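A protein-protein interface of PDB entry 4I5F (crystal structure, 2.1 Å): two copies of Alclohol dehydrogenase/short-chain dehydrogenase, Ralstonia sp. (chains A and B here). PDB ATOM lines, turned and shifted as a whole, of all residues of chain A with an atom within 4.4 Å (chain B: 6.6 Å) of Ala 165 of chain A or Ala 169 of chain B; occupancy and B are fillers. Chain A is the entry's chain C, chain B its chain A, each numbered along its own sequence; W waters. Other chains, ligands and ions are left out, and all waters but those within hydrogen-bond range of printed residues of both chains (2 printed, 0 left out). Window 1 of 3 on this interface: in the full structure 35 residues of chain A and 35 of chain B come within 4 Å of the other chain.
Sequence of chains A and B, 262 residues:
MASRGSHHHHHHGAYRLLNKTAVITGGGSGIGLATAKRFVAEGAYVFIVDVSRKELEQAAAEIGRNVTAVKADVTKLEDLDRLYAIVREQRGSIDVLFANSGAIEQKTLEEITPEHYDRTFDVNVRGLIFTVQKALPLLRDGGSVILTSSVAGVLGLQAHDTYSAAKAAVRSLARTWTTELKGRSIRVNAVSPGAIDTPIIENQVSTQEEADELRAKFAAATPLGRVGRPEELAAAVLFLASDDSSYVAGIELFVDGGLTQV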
ATOM      1  N   PHE A 121     -19.862  -8.133   8.983  1.00  0.00           N
ATOM      2  CA  PHE A 121     -18.776  -7.163   9.120  1.00  0.00           C
ATOM      3  C   PHE A 121     -17.748  -7.055   8.015  1.00  0.00           C
ATOM      4  O   PHE A 121     -17.160  -5.967   7.836  1.00  0.00           O
ATOM      5  CB  PHE A 121     -18.101  -7.338  10.479  1.00  0.00           C
ATOM      6  CG  PHE A 121     -18.884  -6.667  11.584  1.00  0.00           C
ATOM      7  CD1 PHE A 121     -20.076  -7.238  12.056  1.00  0.00           C
ATOM      8  CD2 PHE A 121     -18.492  -5.461  12.092  1.00  0.00           C
ATOM      9  CE1 PHE A 121     -20.836  -6.607  13.050  1.00  0.00           C
ATOM     10  CE2 PHE A 121     -19.294  -4.822  13.075  1.00  0.00           C
ATOM     11  CZ  PHE A 121     -20.461  -5.400  13.534  1.00  0.00           C
ATOM     12  N   ASP A 161     -29.172  -7.209  14.371  1.00  0.00           N
ATOM     13  CA  ASP A 161     -28.110  -6.982  15.282  1.00  0.00           C
ATOM     14  C   ASP A 161     -26.796  -6.585  14.609  1.00  0.00           C
ATOM     15  O   ASP A 161     -26.271  -5.508  14.918  1.00  0.00           O
ATOM     16  CB  ASP A 161     -27.873  -8.175  16.159  1.00  0.00           C
ATOM     17  CG  ASP A 161     -29.134  -8.711  16.822  1.00  0.00           C
ATOM     18  OD1 ASP A 161     -30.183  -8.857  16.140  1.00  0.00           O
ATOM     19  OD2 ASP A 161     -29.060  -9.049  18.041  1.00  0.00           O
ATOM     20  N   THR A 162     -26.264  -7.458  13.704  1.00  0.00           N
ATOM     21  CA  THR A 162     -24.979  -7.182  13.127  1.00  0.00           C
ATOM     22  C   THR A 162     -25.018  -6.084  12.056  1.00  0.00           C
ATOM     23  O   THR A 162     -24.145  -5.198  12.054  1.00  0.00           O
ATOM     24  CB  THR A 162     -24.215  -8.435  12.601  1.00  0.00           C
ATOM     25  OG1 THR A 162     -24.980  -9.043  11.565  1.00  0.00           O
ATOM     26  CG2 THR A 162     -23.961  -9.457  13.742  1.00  0.00           C
ATOM     27  N   TYR A 163     -26.042  -6.107  11.200  1.00  0.00           N
ATOM     28  CA  TYR A 163     -26.192  -5.083  10.169  1.00  0.00           C
ATOM     29  C   TYR A 163     -26.296  -3.708  10.819  1.00  0.00           C
ATOM     30  O   TYR A 163     -25.541  -2.797  10.439  1.00  0.00           O
ATOM     31  CB  TYR A 163     -27.454  -5.319   9.360  1.00  0.00           C
ATOM     32  CG  TYR A 163     -27.648  -4.282   8.304  1.00  0.00           C
ATOM     33  CD1 TYR A 163     -27.023  -4.405   7.070  1.00  0.00           C
ATOM     34  CD2 TYR A 163     -28.438  -3.170   8.549  1.00  0.00           C
ATOM     35  CE1 TYR A 163     -27.247  -3.495   6.069  1.00  0.00           C
ATOM     36  CE2 TYR A 163     -28.677  -2.223   7.549  1.00  0.00           C
ATOM     37  CZ  TYR A 163     -28.066  -2.399   6.323  1.00  0.00           C
ATOM     38  OH  TYR A 163     -28.265  -1.459   5.374  1.00  0.00           O
ATOM     39  N   SER A 164     -27.188  -3.533  11.819  1.00  0.00           N
ATOM     40  CA  SER A 164     -27.257  -2.194  12.441  1.00  0.00           C
ATOM     41  C   SER A 164     -25.878  -1.821  13.056  1.00  0.00           C
ATOM     42  O   SER A 164     -25.399  -0.654  12.902  1.00  0.00           O
ATOM     43  CB  SER A 164     -28.402  -2.117  13.461  1.00  0.00           C
ATOM     44  OG  SER A 164     -29.632  -2.437  12.794  1.00  0.00           O
ATOM     45  N   ALA A 165     -25.240  -2.812  13.734  1.00  0.00           N
ATOM     46  CA  ALA A 165     -24.002  -2.535  14.441  1.00  0.00           C
ATOM     47  C   ALA A 165     -22.941  -2.096  13.447  1.00  0.00           C
ATOM     48  O   ALA A 165     -22.284  -1.092  13.639  1.00  0.00           O
ATOM     49  CB  ALA A 165     -23.592  -3.756  15.258  1.00  0.00           C
ATOM     50  N   ALA A 166     -22.803  -2.827  12.348  1.00  0.00           N
ATOM     51  CA  ALA A 166     -21.851  -2.559  11.297  1.00  0.00           C
ATOM     52  C   ALA A 166     -22.173  -1.195  10.611  1.00  0.00           C
ATOM     53  O   ALA A 166     -21.294  -0.373  10.479  1.00  0.00           O
ATOM     54  CB  ALA A 166     -21.956  -3.692  10.301  1.00  0.00           C
ATOM     55  N   LYS A 167     -23.423  -0.921  10.229  1.00  0.00           N
ATOM     56  CA  LYS A 167     -23.728   0.455   9.737  1.00  0.00           C
ATOM     57  C   LYS A 167     -23.425   1.617  10.683  1.00  0.00           C
ATOM     58  O   LYS A 167     -23.244   2.773  10.194  1.00  0.00           O
ATOM     59  CB  LYS A 167     -25.184   0.599   9.321  1.00  0.00           C
ATOM     60  CG  LYS A 167     -25.579  -0.271   8.125  1.00  0.00           C
ATOM     61  CD  LYS A 167     -24.440  -0.155   7.107  1.00  0.00           C
ATOM     62  CE  LYS A 167     -24.954  -0.636   5.732  1.00  0.00           C
ATOM     63  NZ  LYS A 167     -24.009  -0.248   4.644  1.00  0.00           N
ATOM     64  N   ALA A 168     -23.472   1.387  12.011  1.00  0.00           N
ATOM     65  CA  ALA A 168     -23.040   2.492  12.919  1.00  0.00           C
ATOM     66  C   ALA A 168     -21.524   2.654  12.773  1.00  0.00           C
ATOM     67  O   ALA A 168     -20.998   3.731  12.900  1.00  0.00           O
ATOM     68  CB  ALA A 168     -23.353   2.200  14.411  1.00  0.00           C
ATOM     69  N   ALA A 169     -20.825   1.502  12.631  1.00  0.00           N
ATOM     70  CA  ALA A 169     -19.406   1.529  12.453  1.00  0.00           C
ATOM     71  C   ALA A 169     -19.124   2.421  11.238  1.00  0.00           C
ATOM     72  O   ALA A 169     -18.197   3.168  11.270  1.00  0.00           O
ATOM     73  CB  ALA A 169     -18.858   0.117  12.216  1.00  0.00           C
ATOM     74  N   PHE B 121     -11.751  -5.520  16.194  1.00  0.00           N
ATOM     75  CA  PHE B 121     -13.175  -5.958  16.143  1.00  0.00           C
ATOM     76  C   PHE B 121     -13.529  -7.215  16.964  1.00  0.00           C
ATOM     77  O   PHE B 121     -14.659  -7.301  17.523  1.00  0.00           O
ATOM     78  CB  PHE B 121     -13.670  -5.990  14.690  1.00  0.00           C
ATOM     79  CG  PHE B 121     -14.160  -4.611  14.230  1.00  0.00           C
ATOM     80  CD1 PHE B 121     -13.253  -3.598  13.898  1.00  0.00           C
ATOM     81  CD2 PHE B 121     -15.525  -4.294  14.222  1.00  0.00           C
ATOM     82  CE1 PHE B 121     -13.678  -2.311  13.549  1.00  0.00           C
ATOM     83  CE2 PHE B 121     -15.951  -2.985  13.900  1.00  0.00           C
ATOM     84  CZ  PHE B 121     -15.026  -2.008  13.533  1.00  0.00           C
ATOM     85  N   VAL B 125     -16.008  -6.079  19.627  1.00  0.00           N
ATOM     86  CA  VAL B 125     -17.361  -6.361  19.098  1.00  0.00           C
ATOM     87  C   VAL B 125     -17.687  -7.833  19.117  1.00  0.00           C
ATOM     88  O   VAL B 125     -18.708  -8.219  19.695  1.00  0.00           O
ATOM     89  CB  VAL B 125     -17.575  -5.831  17.670  1.00  0.00           C
ATOM     90  CG1 VAL B 125     -19.072  -5.970  17.214  1.00  0.00           C
ATOM     91  CG2 VAL B 125     -17.169  -4.362  17.617  1.00  0.00           C
ATOM     92  N   LEU B 128     -18.010  -9.397  22.373  1.00  0.00           N
ATOM     93  CA  LEU B 128     -19.069  -8.714  23.133  1.00  0.00           C
ATOM     94  C   LEU B 128     -20.397  -9.301  22.741  1.00  0.00           C
ATOM     95  O   LEU B 128     -21.201  -9.722  23.613  1.00  0.00           O
ATOM     96  CB  LEU B 128     -19.024  -7.232  22.883  1.00  0.00           C
ATOM     97  CG  LEU B 128     -20.289  -6.572  23.511  1.00  0.00           C
ATOM     98  CD1 LEU B 128     -20.136  -6.173  24.949  1.00  0.00           C
ATOM     99  CD2 LEU B 128     -20.716  -5.336  22.771  1.00  0.00           C
ATOM    100  N   ILE B 129     -20.579  -9.512  21.442  1.00  0.00           N
ATOM    101  CA  ILE B 129     -21.763 -10.221  20.955  1.00  0.00           C
ATOM    102  C   ILE B 129     -21.934 -11.609  21.581  1.00  0.00           C
ATOM    103  O   ILE B 129     -22.974 -11.893  22.105  1.00  0.00           O
ATOM    104  CB  ILE B 129     -21.734 -10.359  19.418  1.00  0.00           C
ATOM    105  CG1 ILE B 129     -21.706  -8.925  18.768  1.00  0.00           C
ATOM    106  CG2 ILE B 129     -22.845 -11.303  18.960  1.00  0.00           C
ATOM    107  CD1 ILE B 129     -21.712  -8.824  17.272  1.00  0.00           C
ATOM    108  N   LEU B 147     -23.173  -2.361  28.484  1.00  0.00           N
ATOM    109  CA  LEU B 147     -22.061  -2.469  27.506  1.00  0.00           C
ATOM    110  C   LEU B 147     -21.077  -1.277  27.630  1.00  0.00           C
ATOM    111  O   LEU B 147     -21.469  -0.136  27.841  1.00  0.00           O
ATOM    112  CB  LEU B 147     -22.609  -2.552  26.071  1.00  0.00           C
ATOM    113  CG  LEU B 147     -23.855  -3.470  25.824  1.00  0.00           C
ATOM    114  CD1 LEU B 147     -24.417  -3.275  24.409  1.00  0.00           C
ATOM    115  CD2 LEU B 147     -23.591  -4.954  26.161  1.00  0.00           C
ATOM    116  N   SER B 149     -19.102   1.126  25.834  1.00  0.00           N
ATOM    117  CA  SER B 149     -18.741   1.782  24.634  1.00  0.00           C
ATOM    118  C   SER B 149     -17.614   2.811  25.016  1.00  0.00           C
ATOM    119  O   SER B 149     -16.748   2.557  25.917  1.00  0.00           O
ATOM    120  CB  SER B 149     -20.021   2.425  24.090  1.00  0.00           C
ATOM    121  OG  SER B 149     -19.841   2.857  22.763  1.00  0.00           O
ATOM    122  N   GLY B 153     -16.878   6.523  20.175  1.00  0.00           N
ATOM    123  CA  GLY B 153     -17.997   6.119  19.299  1.00  0.00           C
ATOM    124  C   GLY B 153     -18.864   7.221  18.689  1.00  0.00           C
ATOM    125  O   GLY B 153     -19.748   6.929  17.858  1.00  0.00           O
ATOM    126  N   SER B 164     -12.934   3.463  17.460  1.00  0.00           N
ATOM    127  CA  SER B 164     -14.192   4.265  17.444  1.00  0.00           C
ATOM    128  C   SER B 164     -15.328   3.591  16.679  1.00  0.00           C
ATOM    129  O   SER B 164     -16.493   3.565  17.120  1.00  0.00           O
ATOM    130  CB  SER B 164     -13.939   5.626  16.796  1.00  0.00           C
ATOM    131  OG  SER B 164     -12.790   6.201  17.375  1.00  0.00           O
ATOM    132  N   ALA B 165     -14.986   2.962  15.577  1.00  0.00           N
ATOM    133  CA  ALA B 165     -15.998   2.311  14.724  1.00  0.00           C
ATOM    134  C   ALA B 165     -16.601   1.158  15.484  1.00  0.00           C
ATOM    135  O   ALA B 165     -17.815   0.955  15.487  1.00  0.00           O
ATOM    136  CB  ALA B 165     -15.350   1.841  13.409  1.00  0.00           C
ATOM    137  N   ALA B 166     -15.765   0.424  16.188  1.00  0.00           N
ATOM    138  CA  ALA B 166     -16.155  -0.725  16.992  1.00  0.00           C
ATOM    139  C   ALA B 166     -16.931  -0.228  18.209  1.00  0.00           C
ATOM    140  O   ALA B 166     -18.005  -0.738  18.444  1.00  0.00           O
ATOM    141  CB  ALA B 166     -14.926  -1.570  17.396  1.00  0.00           C
ATOM    142  N   LYS B 167     -16.473   0.811  18.912  1.00  0.00           N
ATOM    143  CA  LYS B 167     -17.338   1.292  19.972  1.00  0.00           C
ATOM    144  C   LYS B 167     -18.693   1.794  19.506  1.00  0.00           C
ATOM    145  O   LYS B 167     -19.651   1.673  20.240  1.00  0.00           O
ATOM    146  CB  LYS B 167     -16.673   2.355  20.881  1.00  0.00           C
ATOM    147  CG  LYS B 167     -15.422   1.764  21.568  1.00  0.00           C
ATOM    148  CD  LYS B 167     -15.846   0.553  22.380  1.00  0.00           C
ATOM    149  CE  LYS B 167     -14.837   0.332  23.510  1.00  0.00           C
ATOM    150  NZ  LYS B 167     -15.310  -0.893  24.198  1.00  0.00           N
ATOM    151  N   ALA B 168     -18.805   2.404  18.314  1.00  0.00           N
ATOM    152  CA  ALA B 168     -20.161   2.843  17.835  1.00  0.00           C
ATOM    153  C   ALA B 168     -21.047   1.575  17.681  1.00  0.00           C
ATOM    154  O   ALA B 168     -22.269   1.596  17.904  1.00  0.00           O
ATOM    155  CB  ALA B 168     -20.045   3.593  16.483  1.00  0.00           C
ATOM    156  N   ALA B 169     -20.440   0.489  17.155  1.00  0.00           N
ATOM    157  CA  ALA B 169     -21.146  -0.745  16.977  1.00  0.00           C
ATOM    158  C   ALA B 169     -21.684  -1.232  18.346  1.00  0.00           C
ATOM    159  O   ALA B 169     -22.794  -1.719  18.445  1.00  0.00           O
ATOM    160  CB  ALA B 169     -20.236  -1.839  16.259  1.00  0.00           C
ATOM    161  N   VAL B 170     -20.855  -1.175  19.372  1.00  0.00           N
ATOM    162  CA  VAL B 170     -21.248  -1.627  20.679  1.00  0.00           C
ATOM    163  C   VAL B 170     -22.487  -0.803  21.099  1.00  0.00           C
ATOM    164  O   VAL B 170     -23.544  -1.367  21.499  1.00  0.00           O
ATOM    165  CB  VAL B 170     -20.021  -1.506  21.711  1.00  0.00           C
ATOM    166  CG1 VAL B 170     -20.492  -1.580  23.212  1.00  0.00           C
ATOM    167  CG2 VAL B 170     -18.987  -2.570  21.397  1.00  0.00           C
ATOM    168  N   ARG B 171     -22.450   0.501  20.882  1.00  0.00           N
ATOM    169  CA  ARG B 171     -23.636   1.379  21.324  1.00  0.00           C
ATOM    170  C   ARG B 171     -24.925   0.933  20.565  1.00  0.00           C
ATOM    171  O   ARG B 171     -26.041   0.932  21.148  1.00  0.00           O
ATOM    172  CB  ARG B 171     -23.375   2.843  21.011  1.00  0.00           C
ATOM    173  CG  ARG B 171     -24.376   3.886  21.549  1.00  0.00           C
ATOM    174  CD  ARG B 171     -25.606   3.987  20.640  1.00  0.00           C
ATOM    175  NE  ARG B 171     -26.681   4.751  21.319  1.00  0.00           N
ATOM    176  CZ  ARG B 171     -27.633   4.239  22.123  1.00  0.00           C
ATOM    177  NH1 ARG B 171     -27.653   2.927  22.467  1.00  0.00           N
ATOM    178  NH2 ARG B 171     -28.541   5.059  22.627  1.00  0.00           N
ATOM    179  N   SER B 172     -24.753   0.454  19.320  1.00  0.00           N
ATOM    180  CA  SER B 172     -25.903   0.147  18.471  1.00  0.00           C
ATOM    181  C   SER B 172     -26.553  -1.144  19.037  1.00  0.00           C
ATOM    182  O   SER B 172     -27.773  -1.260  18.931  1.00  0.00           O
ATOM    183  CB  SER B 172     -25.442  -0.101  16.996  1.00  0.00           C
ATOM    184  OG  SER B 172     -26.527  -0.714  16.246  1.00  0.00           O
ATOM    185  N   LEU B 173     -25.708  -2.085  19.575  1.00  0.00           N
ATOM    186  CA  LEU B 173     -26.136  -3.386  20.154  1.00  0.00           C
ATOM    187  C   LEU B 173     -27.027  -3.162  21.351  1.00  0.00           C
ATOM    188  O   LEU B 173     -28.010  -3.862  21.546  1.00  0.00           O
ATOM    189  CB  LEU B 173     -24.980  -4.411  20.451  1.00  0.00           C
ATOM    190  CG  LEU B 173     -24.229  -4.818  19.164  1.00  0.00           C
ATOM    191  CD1 LEU B 173     -22.821  -5.353  19.323  1.00  0.00           C
ATOM    192  CD2 LEU B 173     -25.082  -5.748  18.233  1.00  0.00           C
ATOM    193  N   ALA B 174     -26.794  -2.114  22.100  1.00  0.00           N
ATOM    194  CA  ALA B 174     -27.758  -1.757  23.197  1.00  0.00           C
ATOM    195  C   ALA B 174     -29.123  -1.529  22.645  1.00  0.00           C
ATOM    196  O   ALA B 174     -30.059  -1.997  23.233  1.00  0.00           O
ATOM    197  CB  ALA B 174     -27.306  -0.571  24.024  1.00  0.00           C
ATOM    198  N   THR B 176     -30.524  -2.630  19.748  1.00  0.00           N
ATOM    199  CA  THR B 176     -31.164  -3.799  19.146  1.00  0.00           C
ATOM    200  C   THR B 176     -31.498  -4.807  20.227  1.00  0.00           C
ATOM    201  O   THR B 176     -32.604  -5.415  20.235  1.00  0.00           O
ATOM    202  CB  THR B 176     -30.190  -4.515  18.182  1.00  0.00           C
ATOM    203  OG1 THR B 176     -29.803  -3.557  17.209  1.00  0.00           O
ATOM    204  CG2 THR B 176     -30.859  -5.742  17.501  1.00  0.00           C
HETATM  205  O   HOH W   1     -31.053  -2.503  15.425  1.00  0.00           O
HETATM  206  O   HOH W   2     -27.212  -3.774  16.535  1.00  0.00           O
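Phe 121 of chain A touches Phe 121 of chain B. CZ of Phe 121 of chain A touches CG1 of Val 125 of chain B, 3.97 Å away. Asp 161 of chain A touches Leu 173 of chain B. Thr 176 of chain B touches Asp 161 of chain A. C of Ser 164 of chain A touches OG of Ser 172 of chain B (3.4 Å). O of Ala 165 of chain A touches CB of Ala 169 of chain B (3.4 Å). Ala 165 of chain A touches Ser 172 of chain B (N to OG, 3.5 Å). Ala 165 of chain A touches Leu 173 of chain B. O of Ala 168 of chain B touches CB of Ala 168 of chain A, 3.7 Å away. Ala 169 of chain A touches Ala 165 of chain B.
Ala 165 of chain A touches just these residues of chain B: Ala 169 (3.4 Å), Ser 172 (3.5 Å) and Leu 173 (3.9 Å). Of the printed residues of chain A, Ala 169 of chain B touches Ala 165 (3.4 Å). Printed residues of chain A within 4 Å of Val 125 of chain B: Phe 121. Of the printed residues of chain B, Ala 168 of chain A touches Ala 168. Printed residues of chain A within 4 Å of Leu 173 of chain B: Asp 161 (3.5 Å) and Ala 165 (3.9 Å). Lys 167 of chain B touches none of the printed residues of chain A. The nearest residue of chain B that does not touch Ala 165 of chain A is Ala 168 of chain B (5.0 Å). The nearest printed residue of chain A that does not touch Ala 169 of chain B is Ala 168 of chain A (4.4 Å). The nearest printed residue of chain A that does not touch Ala 165 of chain B is Ala 168 of chain A (4.9 Å).
Printed residues of chain A that touch a printed residue of chain B: Phe 121, Asp 161, Ser 164, Ala 165, Ala 168 and Ala 169. Hydrophobic or aromatic side chains of chain A that line the printed part of chain B: Phe 121, Ala 165, Ala 168 and Ala 169. Of the 19 printed residues of chain B, 8 touch a printed residue of chain A. Hydrophobic or aromatic side chains of chain B that line the printed part of chain A: Phe 121, Val 125, Ala 165, Ala 168, Ala 169 and Leu 173.
Phe 121 of chain B touches its own counterpart, Phe 121 of chain A. Ala 165 of chain A touches Ala 169 of chain B, and with the chains exchanged Ala 169 of chain A touches Ala 165 of chain B. Ala 168 of chain A touches its own counterpart, Ala 168 of chain B. Positions printed for both chains: 121, 164, 165, 166, 167, 168 and 169. Of the 10 pairs that touch across the chains among the printed residues, 4 have their exchanged pair printed and touching as well.
Water W1 bridges the side-chain hydroxyl (OG1) of Thr 176 of chain B and the side-chain hydroxyl (OG) of Ser 164 of chain A. Water W2 lies within hydrogen-bond range of O of Asp 161 of chain A, OG1 of Thr 176 of chain B and OG of Ser 172 of chain B.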
